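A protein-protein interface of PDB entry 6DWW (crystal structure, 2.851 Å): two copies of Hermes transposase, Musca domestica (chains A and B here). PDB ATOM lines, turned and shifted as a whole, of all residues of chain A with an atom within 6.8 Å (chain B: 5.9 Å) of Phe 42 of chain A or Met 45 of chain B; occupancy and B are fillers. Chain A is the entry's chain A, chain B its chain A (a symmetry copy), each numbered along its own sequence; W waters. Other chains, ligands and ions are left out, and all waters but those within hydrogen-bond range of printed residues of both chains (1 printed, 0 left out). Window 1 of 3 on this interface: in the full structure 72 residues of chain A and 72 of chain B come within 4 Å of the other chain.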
ATOM      1  N   ALA A  19      10.425   0.533  23.580  1.00  0.00           N
ATOM      2  CA  ALA A  19      10.784  -0.848  23.875  1.00  0.00           C
ATOM      3  C   ALA A  19      10.671  -1.163  25.360  1.00  0.00           C
ATOM      4  O   ALA A  19      10.297  -2.282  25.722  1.00  0.00           O
ATOM      5  CB  ALA A  19      12.199  -1.147  23.384  1.00  0.00           C
ATOM      6  N   LYS A  22       6.789  -1.683  25.909  1.00  0.00           N
ATOM      7  CA  LYS A  22       6.237  -2.975  25.521  1.00  0.00           C
ATOM      8  C   LYS A  22       6.776  -4.114  26.378  1.00  0.00           C
ATOM      9  O   LYS A  22       6.094  -5.136  26.526  1.00  0.00           O
ATOM     10  CB  LYS A  22       6.517  -3.253  24.038  1.00  0.00           C
ATOM     11  CG  LYS A  22       6.088  -2.133  23.083  1.00  0.00           C
ATOM     12  CD  LYS A  22       4.764  -2.428  22.370  1.00  0.00           C
ATOM     13  CE  LYS A  22       3.633  -1.517  22.846  1.00  0.00           C
ATOM     14  NZ  LYS A  22       3.952  -0.064  22.708  1.00  0.00           N
ATOM     15  N   CYS A  23       7.979  -3.963  26.942  1.00  0.00           N
ATOM     16  CA  CYS A  23       8.498  -4.971  27.863  1.00  0.00           C
ATOM     17  C   CYS A  23       7.800  -4.891  29.215  1.00  0.00           C
ATOM     18  O   CYS A  23       7.452  -5.922  29.804  1.00  0.00           O
ATOM     19  CB  CYS A  23      10.008  -4.810  28.030  1.00  0.00           C
ATOM     20  SG  CYS A  23      10.996  -5.381  26.617  1.00  0.00           S
ATOM     21  N   ALA A  24       7.577  -3.675  29.717  1.00  0.00           N
ATOM     22  CA  ALA A  24       6.875  -3.524  30.986  1.00  0.00           C
ATOM     23  C   ALA A  24       5.459  -4.080  30.908  1.00  0.00           C
ATOM     24  O   ALA A  24       4.966  -4.675  31.873  1.00  0.00           O
ATOM     25  CB  ALA A  24       6.849  -2.055  31.402  1.00  0.00           C
ATOM     26  N   TRP A  26       4.465  -6.541  28.994  1.00  0.00           N
ATOM     27  CA  TRP A  26       4.513  -7.998  28.938  1.00  0.00           C
ATOM     28  C   TRP A  26       4.619  -8.591  30.334  1.00  0.00           C
ATOM     29  O   TRP A  26       3.912  -9.548  30.671  1.00  0.00           O
ATOM     30  CB  TRP A  26       5.682  -8.444  28.063  1.00  0.00           C
ATOM     31  CG  TRP A  26       6.107  -9.865  28.267  1.00  0.00           C
ATOM     32  CD1 TRP A  26       5.324 -10.979  28.175  1.00  0.00           C
ATOM     33  CD2 TRP A  26       7.429 -10.327  28.572  1.00  0.00           C
ATOM     34  NE1 TRP A  26       6.074 -12.106  28.415  1.00  0.00           N
ATOM     35  CE2 TRP A  26       7.369 -11.733  28.660  1.00  0.00           C
ATOM     36  CE3 TRP A  26       8.657  -9.689  28.781  1.00  0.00           C
ATOM     37  CZ2 TRP A  26       8.488 -12.510  28.948  1.00  0.00           C
ATOM     38  CZ3 TRP A  26       9.768 -10.465  29.066  1.00  0.00           C
ATOM     39  CH2 TRP A  26       9.676 -11.859  29.148  1.00  0.00           C
ATOM     40  N   VAL A  27       5.497  -8.026  31.164  1.00  0.00           N
ATOM     41  CA  VAL A  27       5.672  -8.508  32.531  1.00  0.00           C
ATOM     42  C   VAL A  27       4.401  -8.296  33.343  1.00  0.00           C
ATOM     43  O   VAL A  27       4.026  -9.133  34.175  1.00  0.00           O
ATOM     44  CB  VAL A  27       6.890  -7.812  33.171  1.00  0.00           C
ATOM     45  CG1 VAL A  27       6.697  -7.618  34.663  1.00  0.00           C
ATOM     46  CG2 VAL A  27       8.156  -8.606  32.884  1.00  0.00           C
ATOM     47  N   ALA A  36      12.979 -11.586  33.772  1.00  0.00           N
ATOM     48  CA  ALA A  36      12.774 -12.313  32.525  1.00  0.00           C
ATOM     49  C   ALA A  36      13.303 -11.547  31.317  1.00  0.00           C
ATOM     50  O   ALA A  36      13.524 -12.154  30.263  1.00  0.00           O
ATOM     51  CB  ALA A  36      11.290 -12.600  32.317  1.00  0.00           C
ATOM     52  N   VAL A  37      13.514 -10.233  31.443  1.00  0.00           N
ATOM     53  CA  VAL A  37      13.874  -9.381  30.320  1.00  0.00           C
ATOM     54  C   VAL A  37      15.364  -9.531  30.052  1.00  0.00           C
ATOM     55  O   VAL A  37      15.902  -8.921  29.126  1.00  0.00           O
ATOM     56  CB  VAL A  37      13.487  -7.922  30.613  1.00  0.00           C
ATOM     57  CG1 VAL A  37      14.449  -7.307  31.634  1.00  0.00           C
ATOM     58  CG2 VAL A  37      13.429  -7.109  29.330  1.00  0.00           C
ATOM     59  N   SER A  38      16.035 -10.368  30.846  1.00  0.00           N
ATOM     60  CA  SER A  38      17.485 -10.496  30.787  1.00  0.00           C
ATOM     61  C   SER A  38      17.949 -11.946  30.709  1.00  0.00           C
ATOM     62  O   SER A  38      19.140 -12.211  30.884  1.00  0.00           O
ATOM     63  CB  SER A  38      18.130  -9.792  31.993  1.00  0.00           C
ATOM     64  OG  SER A  38      17.766 -10.402  33.219  1.00  0.00           O
ATOM     65  N   GLY A  39      17.049 -12.884  30.444  1.00  0.00           N
ATOM     66  CA  GLY A  39      17.464 -14.259  30.268  1.00  0.00           C
ATOM     67  C   GLY A  39      18.334 -14.432  29.037  1.00  0.00           C
ATOM     68  O   GLY A  39      18.153 -13.768  28.017  1.00  0.00           O
ATOM     69  N   SER A  40      19.307 -15.345  29.143  1.00  0.00           N
ATOM     70  CA  SER A  40      20.179 -15.633  28.006  1.00  0.00           C
ATOM     71  C   SER A  40      19.371 -16.095  26.799  1.00  0.00           C
ATOM     72  O   SER A  40      19.679 -15.729  25.656  1.00  0.00           O
ATOM     73  CB  SER A  40      21.217 -16.694  28.386  1.00  0.00           C
ATOM     74  OG  SER A  40      22.082 -16.237  29.414  1.00  0.00           O
ATOM     75  N   GLY A  41      18.326 -16.897  27.033  1.00  0.00           N
ATOM     76  CA  GLY A  41      17.503 -17.366  25.936  1.00  0.00           C
ATOM     77  C   GLY A  41      16.502 -16.341  25.456  1.00  0.00           C
ATOM     78  O   GLY A  41      16.063 -16.395  24.305  1.00  0.00           O
ATOM     79  N   PHE A  42      16.122 -15.401  26.321  1.00  0.00           N
ATOM     80  CA  PHE A  42      15.232 -14.330  25.893  1.00  0.00           C
ATOM     81  C   PHE A  42      15.932 -13.407  24.907  1.00  0.00           C
ATOM     82  O   PHE A  42      15.360 -13.032  23.876  1.00  0.00           O
ATOM     83  CB  PHE A  42      14.738 -13.544  27.100  1.00  0.00           C
ATOM     84  CG  PHE A  42      13.791 -12.435  26.752  1.00  0.00           C
ATOM     85  CD1 PHE A  42      12.482 -12.714  26.393  1.00  0.00           C
ATOM     86  CD2 PHE A  42      14.203 -11.114  26.798  1.00  0.00           C
ATOM     87  CE1 PHE A  42      11.603 -11.696  26.081  1.00  0.00           C
ATOM     88  CE2 PHE A  42      13.331 -10.089  26.486  1.00  0.00           C
ATOM     89  CZ  PHE A  42      12.029 -10.380  26.125  1.00  0.00           C
ATOM     90  N   ILE A  43      17.177 -13.035  25.211  1.00  0.00           N
ATOM     91  CA  ILE A  43      17.944 -12.163  24.325  1.00  0.00           C
ATOM     92  C   ILE A  43      18.218 -12.860  22.995  1.00  0.00           C
ATOM     93  O   ILE A  43      18.002 -12.288  21.920  1.00  0.00           O
ATOM     94  CB  ILE A  43      19.244 -11.717  25.016  1.00  0.00           C
ATOM     95  CG1 ILE A  43      18.927 -10.950  26.302  1.00  0.00           C
ATOM     96  CG2 ILE A  43      20.074 -10.854  24.091  1.00  0.00           C
ATOM     97  CD1 ILE A  43      20.151 -10.392  26.991  1.00  0.00           C
ATOM     98  N   ASP A  44      18.686 -14.113  23.044  1.00  0.00           N
ATOM     99  CA  ASP A  44      18.928 -14.856  21.810  1.00  0.00           C
ATOM    100  C   ASP A  44      17.656 -15.012  20.982  1.00  0.00           C
ATOM    101  O   ASP A  44      17.726 -15.130  19.754  1.00  0.00           O
ATOM    102  CB  ASP A  44      19.525 -16.232  22.120  1.00  0.00           C
ATOM    103  CG  ASP A  44      20.997 -16.166  22.489  1.00  0.00           C
ATOM    104  OD1 ASP A  44      21.495 -15.057  22.775  1.00  0.00           O
ATOM    105  OD2 ASP A  44      21.653 -17.232  22.502  1.00  0.00           O
ATOM    106  N   MET A  45      16.489 -15.013  21.628  1.00  0.00           N
ATOM    107  CA  MET A  45      15.237 -15.122  20.889  1.00  0.00           C
ATOM    108  C   MET A  45      14.838 -13.791  20.261  1.00  0.00           C
ATOM    109  O   MET A  45      14.355 -13.760  19.125  1.00  0.00           O
ATOM    110  CB  MET A  45      14.127 -15.633  21.809  1.00  0.00           C
ATOM    111  CG  MET A  45      12.785 -15.816  21.125  1.00  0.00           C
ATOM    112  SD  MET A  45      11.445 -16.192  22.272  1.00  0.00           S
ATOM    113  CE  MET A  45      11.469 -14.735  23.317  1.00  0.00           C
ATOM    114  N   ILE A  46      15.034 -12.684  20.982  1.00  0.00           N
ATOM    115  CA  ILE A  46      14.684 -11.372  20.442  1.00  0.00           C
ATOM    116  C   ILE A  46      15.560 -11.040  19.237  1.00  0.00           C
ATOM    117  O   ILE A  46      15.106 -10.407  18.276  1.00  0.00           O
ATOM    118  CB  ILE A  46      14.790 -10.295  21.541  1.00  0.00           C
ATOM    119  CG1 ILE A  46      13.756 -10.549  22.637  1.00  0.00           C
ATOM    120  CG2 ILE A  46      14.601  -8.902  20.965  1.00  0.00           C
ATOM    121  CD1 ILE A  46      12.348 -10.656  22.121  1.00  0.00           C
ATOM    122  N   LYS A  47      16.822 -11.475  19.264  1.00  0.00           N
ATOM    123  CA  LYS A  47      17.709 -11.238  18.129  1.00  0.00           C
ATOM    124  C   LYS A  47      17.180 -11.913  16.869  1.00  0.00           C
ATOM    125  O   LYS A  47      17.299 -11.366  15.766  1.00  0.00           O
ATOM    126  CB  LYS A  47      19.123 -11.724  18.457  1.00  0.00           C
ATOM    127  CG  LYS A  47      19.836 -10.861  19.491  1.00  0.00           C
ATOM    128  CD  LYS A  47      21.229 -11.368  19.826  1.00  0.00           C
ATOM    129  CE  LYS A  47      21.904 -10.455  20.847  1.00  0.00           C
ATOM    130  NZ  LYS A  47      23.205 -10.986  21.351  1.00  0.00           N
ATOM    131  N   TRP B  26      14.396 -20.728  24.688  1.00  0.00           N
ATOM    132  CA  TRP B  26      14.148 -19.698  25.691  1.00  0.00           C
ATOM    133  C   TRP B  26      13.487 -20.292  26.926  1.00  0.00           C
ATOM    134  O   TRP B  26      13.885 -19.998  28.059  1.00  0.00           O
ATOM    135  CB  TRP B  26      13.289 -18.587  25.092  1.00  0.00           C
ATOM    136  CG  TRP B  26      12.609 -17.713  26.098  1.00  0.00           C
ATOM    137  CD1 TRP B  26      13.198 -17.014  27.112  1.00  0.00           C
ATOM    138  CD2 TRP B  26      11.209 -17.419  26.170  1.00  0.00           C
ATOM    139  NE1 TRP B  26      12.249 -16.313  27.818  1.00  0.00           N
ATOM    140  CE2 TRP B  26      11.020 -16.545  27.259  1.00  0.00           C
ATOM    141  CE3 TRP B  26      10.095 -17.813  25.420  1.00  0.00           C
ATOM    142  CZ2 TRP B  26       9.765 -16.058  27.616  1.00  0.00           C
ATOM    143  CZ3 TRP B  26       8.848 -17.328  25.777  1.00  0.00           C
ATOM    144  CH2 TRP B  26       8.693 -16.462  26.866  1.00  0.00           C
ATOM    145  N   ASP B  30      15.908 -20.257  30.383  1.00  0.00           N
ATOM    146  CA  ASP B  30      15.436 -19.338  31.408  1.00  0.00           C
ATOM    147  C   ASP B  30      14.403 -19.959  32.339  1.00  0.00           C
ATOM    148  O   ASP B  30      13.938 -19.279  33.262  1.00  0.00           O
ATOM    149  CB  ASP B  30      14.860 -18.079  30.753  1.00  0.00           C
ATOM    150  CG  ASP B  30      15.874 -17.364  29.880  1.00  0.00           C
ATOM    151  OD1 ASP B  30      17.078 -17.689  29.973  1.00  0.00           O
ATOM    152  OD2 ASP B  30      15.468 -16.471  29.108  1.00  0.00           O
ATOM    153  N   SER B  40      -0.782 -12.642  26.130  1.00  0.00           N
ATOM    154  CA  SER B  40      -1.251 -11.493  25.358  1.00  0.00           C
ATOM    155  C   SER B  40      -0.164 -10.431  25.237  1.00  0.00           C
ATOM    156  O   SER B  40      -0.008  -9.805  24.180  1.00  0.00           O
ATOM    157  CB  SER B  40      -2.506 -10.894  26.003  1.00  0.00           C
ATOM    158  OG  SER B  40      -3.586 -11.814  26.001  1.00  0.00           O
ATOM    159  N   GLY B  41       0.606 -10.220  26.310  1.00  0.00           N
ATOM    160  CA  GLY B  41       1.670  -9.235  26.267  1.00  0.00           C
ATOM    161  C   GLY B  41       2.917  -9.732  25.575  1.00  0.00           C
ATOM    162  O   GLY B  41       3.706  -8.931  25.068  1.00  0.00           O
ATOM    163  N   PHE B  42       3.121 -11.049  25.545  1.00  0.00           N
ATOM    164  CA  PHE B  42       4.256 -11.596  24.813  1.00  0.00           C
ATOM    165  C   PHE B  42       4.079 -11.399  23.315  1.00  0.00           C
ATOM    166  O   PHE B  42       5.015 -10.994  22.615  1.00  0.00           O
ATOM    167  CB  PHE B  42       4.426 -13.074  25.140  1.00  0.00           C
ATOM    168  CG  PHE B  42       5.593 -13.714  24.448  1.00  0.00           C
ATOM    169  CD1 PHE B  42       6.887 -13.466  24.875  1.00  0.00           C
ATOM    170  CD2 PHE B  42       5.395 -14.575  23.381  1.00  0.00           C
ATOM    171  CE1 PHE B  42       7.964 -14.061  24.248  1.00  0.00           C
ATOM    172  CE2 PHE B  42       6.467 -15.173  22.746  1.00  0.00           C
ATOM    173  CZ  PHE B  42       7.754 -14.914  23.179  1.00  0.00           C
ATOM    174  N   ILE B  43       2.877 -11.680  22.809  1.00  0.00           N
ATOM    175  CA  ILE B  43       2.596 -11.510  21.386  1.00  0.00           C
ATOM    176  C   ILE B  43       2.684 -10.037  20.995  1.00  0.00           C
ATOM    177  O   ILE B  43       3.335  -9.679  20.007  1.00  0.00           O
ATOM    178  CB  ILE B  43       1.223 -12.113  21.040  1.00  0.00           C
ATOM    179  CG1 ILE B  43       1.200 -13.608  21.369  1.00  0.00           C
ATOM    180  CG2 ILE B  43       0.896 -11.899  19.579  1.00  0.00           C
ATOM    181  CD1 ILE B  43      -0.084 -14.296  20.967  1.00  0.00           C
ATOM    182  N   ASP B  44       2.042  -9.158  21.772  1.00  0.00           N
ATOM    183  CA  ASP B  44       2.121  -7.728  21.484  1.00  0.00           C
ATOM    184  C   ASP B  44       3.559  -7.218  21.527  1.00  0.00           C
ATOM    185  O   ASP B  44       3.890  -6.240  20.848  1.00  0.00           O
ATOM    186  CB  ASP B  44       1.252  -6.934  22.464  1.00  0.00           C
ATOM    187  CG  ASP B  44      -0.229  -7.021  22.142  1.00  0.00           C
ATOM    188  OD1 ASP B  44      -0.620  -7.899  21.344  1.00  0.00           O
ATOM    189  OD2 ASP B  44      -1.005  -6.212  22.698  1.00  0.00           O
ATOM    190  N   MET B  45       4.424  -7.862  22.311  1.00  0.00           N
ATOM    191  CA  MET B  45       5.820  -7.445  22.367  1.00  0.00           C
ATOM    192  C   MET B  45       6.605  -7.949  21.161  1.00  0.00           C
ATOM    193  O   MET B  45       7.442  -7.222  20.616  1.00  0.00           O
ATOM    194  CB  MET B  45       6.462  -7.935  23.666  1.00  0.00           C
ATOM    195  CG  MET B  45       7.913  -7.521  23.839  1.00  0.00           C
ATOM    196  SD  MET B  45       8.712  -8.301  25.255  1.00  0.00           S
ATOM    197  CE  MET B  45       8.559 -10.034  24.823  1.00  0.00           C
ATOM    198  N   ILE B  46       6.349  -9.186  20.729  1.00  0.00           N
ATOM    199  CA  ILE B  46       7.056  -9.734  19.573  1.00  0.00           C
ATOM    200  C   ILE B  46       6.700  -8.953  18.312  1.00  0.00           C
ATOM    201  O   ILE B  46       7.543  -8.754  17.428  1.00  0.00           O
ATOM    202  CB  ILE B  46       6.750 -11.237  19.422  1.00  0.00           C
ATOM    203  CG1 ILE B  46       7.302 -12.016  20.615  1.00  0.00           C
ATOM    204  CG2 ILE B  46       7.333 -11.789  18.132  1.00  0.00           C
ATOM    205  CD1 ILE B  46       8.768 -11.786  20.857  1.00  0.00           C
ATOM    206  N   LYS B  47       5.452  -8.487  18.216  1.00  0.00           N
ATOM    207  CA  LYS B  47       5.048  -7.691  17.061  1.00  0.00           C
ATOM    208  C   LYS B  47       5.861  -6.406  16.967  1.00  0.00           C
ATOM    209  O   LYS B  47       6.206  -5.959  15.868  1.00  0.00           O
ATOM    210  CB  LYS B  47       3.549  -7.386  17.132  1.00  0.00           C
ATOM    211  CG  LYS B  47       2.669  -8.606  16.891  1.00  0.00           C
ATOM    212  CD  LYS B  47       1.185  -8.294  16.990  1.00  0.00           C
ATOM    213  CE  LYS B  47       0.353  -9.545  16.717  1.00  0.00           C
ATOM    214  NZ  LYS B  47      -1.107  -9.353  16.965  1.00  0.00           N
ATOM    215  N   PHE B  48       6.190  -5.808  18.113  1.00  0.00           N
ATOM    216  CA  PHE B  48       7.005  -4.598  18.112  1.00  0.00           C
ATOM    217  C   PHE B  48       8.431  -4.883  17.663  1.00  0.00           C
ATOM    218  O   PHE B  48       9.046  -4.058  16.979  1.00  0.00           O
ATOM    219  CB  PHE B  48       7.006  -3.966  19.500  1.00  0.00           C
ATOM    220  CG  PHE B  48       8.133  -2.995  19.724  1.00  0.00           C
ATOM    221  CD1 PHE B  48       8.021  -1.677  19.313  1.00  0.00           C
ATOM    222  CD2 PHE B  48       9.301  -3.399  20.355  1.00  0.00           C
ATOM    223  CE1 PHE B  48       9.052  -0.778  19.522  1.00  0.00           C
ATOM    224  CE2 PHE B  48      10.337  -2.506  20.565  1.00  0.00           C
ATOM    225  CZ  PHE B  48      10.212  -1.194  20.149  1.00  0.00           C
ATOM    226  N   PHE B  49       8.985  -6.029  18.054  1.00  0.00           N
ATOM    227  CA  PHE B  49      10.383  -6.296  17.740  1.00  0.00           C
ATOM    228  C   PHE B  49      10.603  -6.650  16.274  1.00  0.00           C
ATOM    229  O   PHE B  49      11.719  -6.480  15.773  1.00  0.00           O
ATOM    230  CB  PHE B  49      10.929  -7.400  18.647  1.00  0.00           C
ATOM    231  CG  PHE B  49      11.352  -6.908  20.009  1.00  0.00           C
ATOM    232  CD1 PHE B  49      12.116  -5.759  20.139  1.00  0.00           C
ATOM    233  CD2 PHE B  49      10.969  -7.583  21.158  1.00  0.00           C
ATOM    234  CE1 PHE B  49      12.501  -5.301  21.386  1.00  0.00           C
ATOM    235  CE2 PHE B  49      11.349  -7.130  22.402  1.00  0.00           C
ATOM    236  CZ  PHE B  49      12.116  -5.986  22.518  1.00  0.00           C
ATOM    237  N   ILE B  50       9.579  -7.126  15.566  1.00  0.00           N
ATOM    238  CA  ILE B  50       9.742  -7.291  14.126  1.00  0.00           C
ATOM    239  C   ILE B  50       9.675  -5.947  13.413  1.00  0.00           C
ATOM    240  O   ILE B  50      10.212  -5.814  12.308  1.00  0.00           O
ATOM    241  CB  ILE B  50       8.711  -8.267  13.532  1.00  0.00           C
ATOM    242  CG1 ILE B  50       7.345  -7.600  13.387  1.00  0.00           C
ATOM    243  CG2 ILE B  50       8.609  -9.528  14.388  1.00  0.00           C
ATOM    244  CD1 ILE B  50       6.417  -8.326  12.438  1.00  0.00           C
ATOM    245  N   LEU B  66      17.406  -3.518  24.740  1.00  0.00           N
ATOM    246  CA  LEU B  66      16.603  -4.123  25.794  1.00  0.00           C
ATOM    247  C   LEU B  66      16.803  -3.385  27.116  1.00  0.00           C
ATOM    248  O   LEU B  66      17.923  -2.965  27.435  1.00  0.00           O
ATOM    249  CB  LEU B  66      16.968  -5.597  25.970  1.00  0.00           C
ATOM    250  CG  LEU B  66      16.381  -6.561  24.943  1.00  0.00           C
ATOM    251  CD1 LEU B  66      16.750  -8.003  25.279  1.00  0.00           C
ATOM    252  CD2 LEU B  66      14.872  -6.383  24.867  1.00  0.00           C
HETATM  253  O   HOH W   1      19.723 -17.634  31.224  1.00  0.00           O
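Of the printed residues of chain A, Met 45 of chain B touches Cys 23 (3.9 Å), Trp 26 (3.8 Å) and Phe 42 (3.7 Å).
Of the printed residues of chain A, Asp 30 of chain B touches Gly 39 (3.2 Å), Ser 40 (3.3 Å), Gly 41 (3.3 Å) and Phe 42 (3.1 Å).
Printed residues of chain B within 4 Å of Trp 26 of chain A: Trp 26 (3.999 Å), Gly 41 (3.6 Å), Phe 42 (3.4 Å) and Met 45 (3.8 Å).
Printed residues of chain A within 4 Å of Phe 42 of chain B: Trp 26 and Met 45.
Ala 24 of chain A touches none of the printed residues of chain B.
The nearest residue of chain B that does not touch Phe 42 of chain A is Leu 66 of chain B (4.2 Å).
The nearest printed residue of chain A that does not touch Asp 30 of chain B is Ala 36 of chain A (4.9 Å).
Among the printed residues, pairs that only touch across the chains: Ala 19 of chain A with Phe 48 of chain B, Lys 22 of chain A with Phe 48 of chain B, Cys 23 of chain A with Met 45 of chain B, Trp 26 of chain A with Trp 26 of chain B, Trp 26 of chain A with Gly 41 of chain B, Trp 26 of chain A with Phe 42 of chain B, Trp 26 of chain A with Met 45 of chain B, Gly 39 of chain A with Asp 30 of chain B, Gly 41 of chain A with Trp 26 of chain B, Phe 42 of chain A with Trp 26 of chain B, Phe 42 of chain A with Met 45 of chain B, Ile 43 of chain A with Leu 66 of chain B, Met 45 of chain A with Trp 26 of chain B, Met 45 of chain A with Phe 42 of chain B, Ile 46 of chain A with Ile 46 of chain B and Ile 46 of chain A with Phe 49 of chain B.
Water W1 lies within hydrogen-bond range of OD1 of Asp 30 of chain B (2.9 Å) and N of Ser 40 of chain A (3.1 Å).
The backbone carbonyl oxygen (O) of Ala 19 of chain A lies within hydrogen-bond range of the side-chain sulfur (SG) of Cys 23 of chain A, at 3.3 Å.
OD2 of Asp 30 of chain B lies close to NE1 of Trp 26 of chain B (3.5 Å).
Trp 26 of chain B touches its own counterpart, Trp 26 of chain A.
Trp 26 of chain A touches Gly 41 of chain B, and with the chains exchanged Gly 41 of chain A touches Trp 26 of chain B.
Trp 26 of chain A touches Met 45 of chain B, and with the chains exchanged Met 45 of chain A touches Trp 26 of chain B.
Ile 46 of chain A touches its own counterpart, Ile 46 of chain B.
9 positions are printed for both chains.
The backbone NH (N) of Phe 42 of chain A sits at hydrogen-bond distance from the side-chain carboxylate (OD2) of Asp 30 of chain B (3.1 Å).
OD1 of Asp 30 of chain B sits at hydrogen-bond distance from N of Ser 40 of chain A, at 3.3 Å.
OD1 of Asp 30 of chain B sits at hydrogen-bond distance from N of Gly 41 of chain A, 3.3 Å away.
Printed residues of chain B that touch a printed residue of chain A: Trp 26, Asp 30, Gly 41, Phe 42, Met 45, Ile 46, Phe 48, Phe 49 and Leu 66.
Of the 18 printed residues of chain A, 11 touch a printed residue of chain B.
Among the printed residues, 19 pairs touch across the chains.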
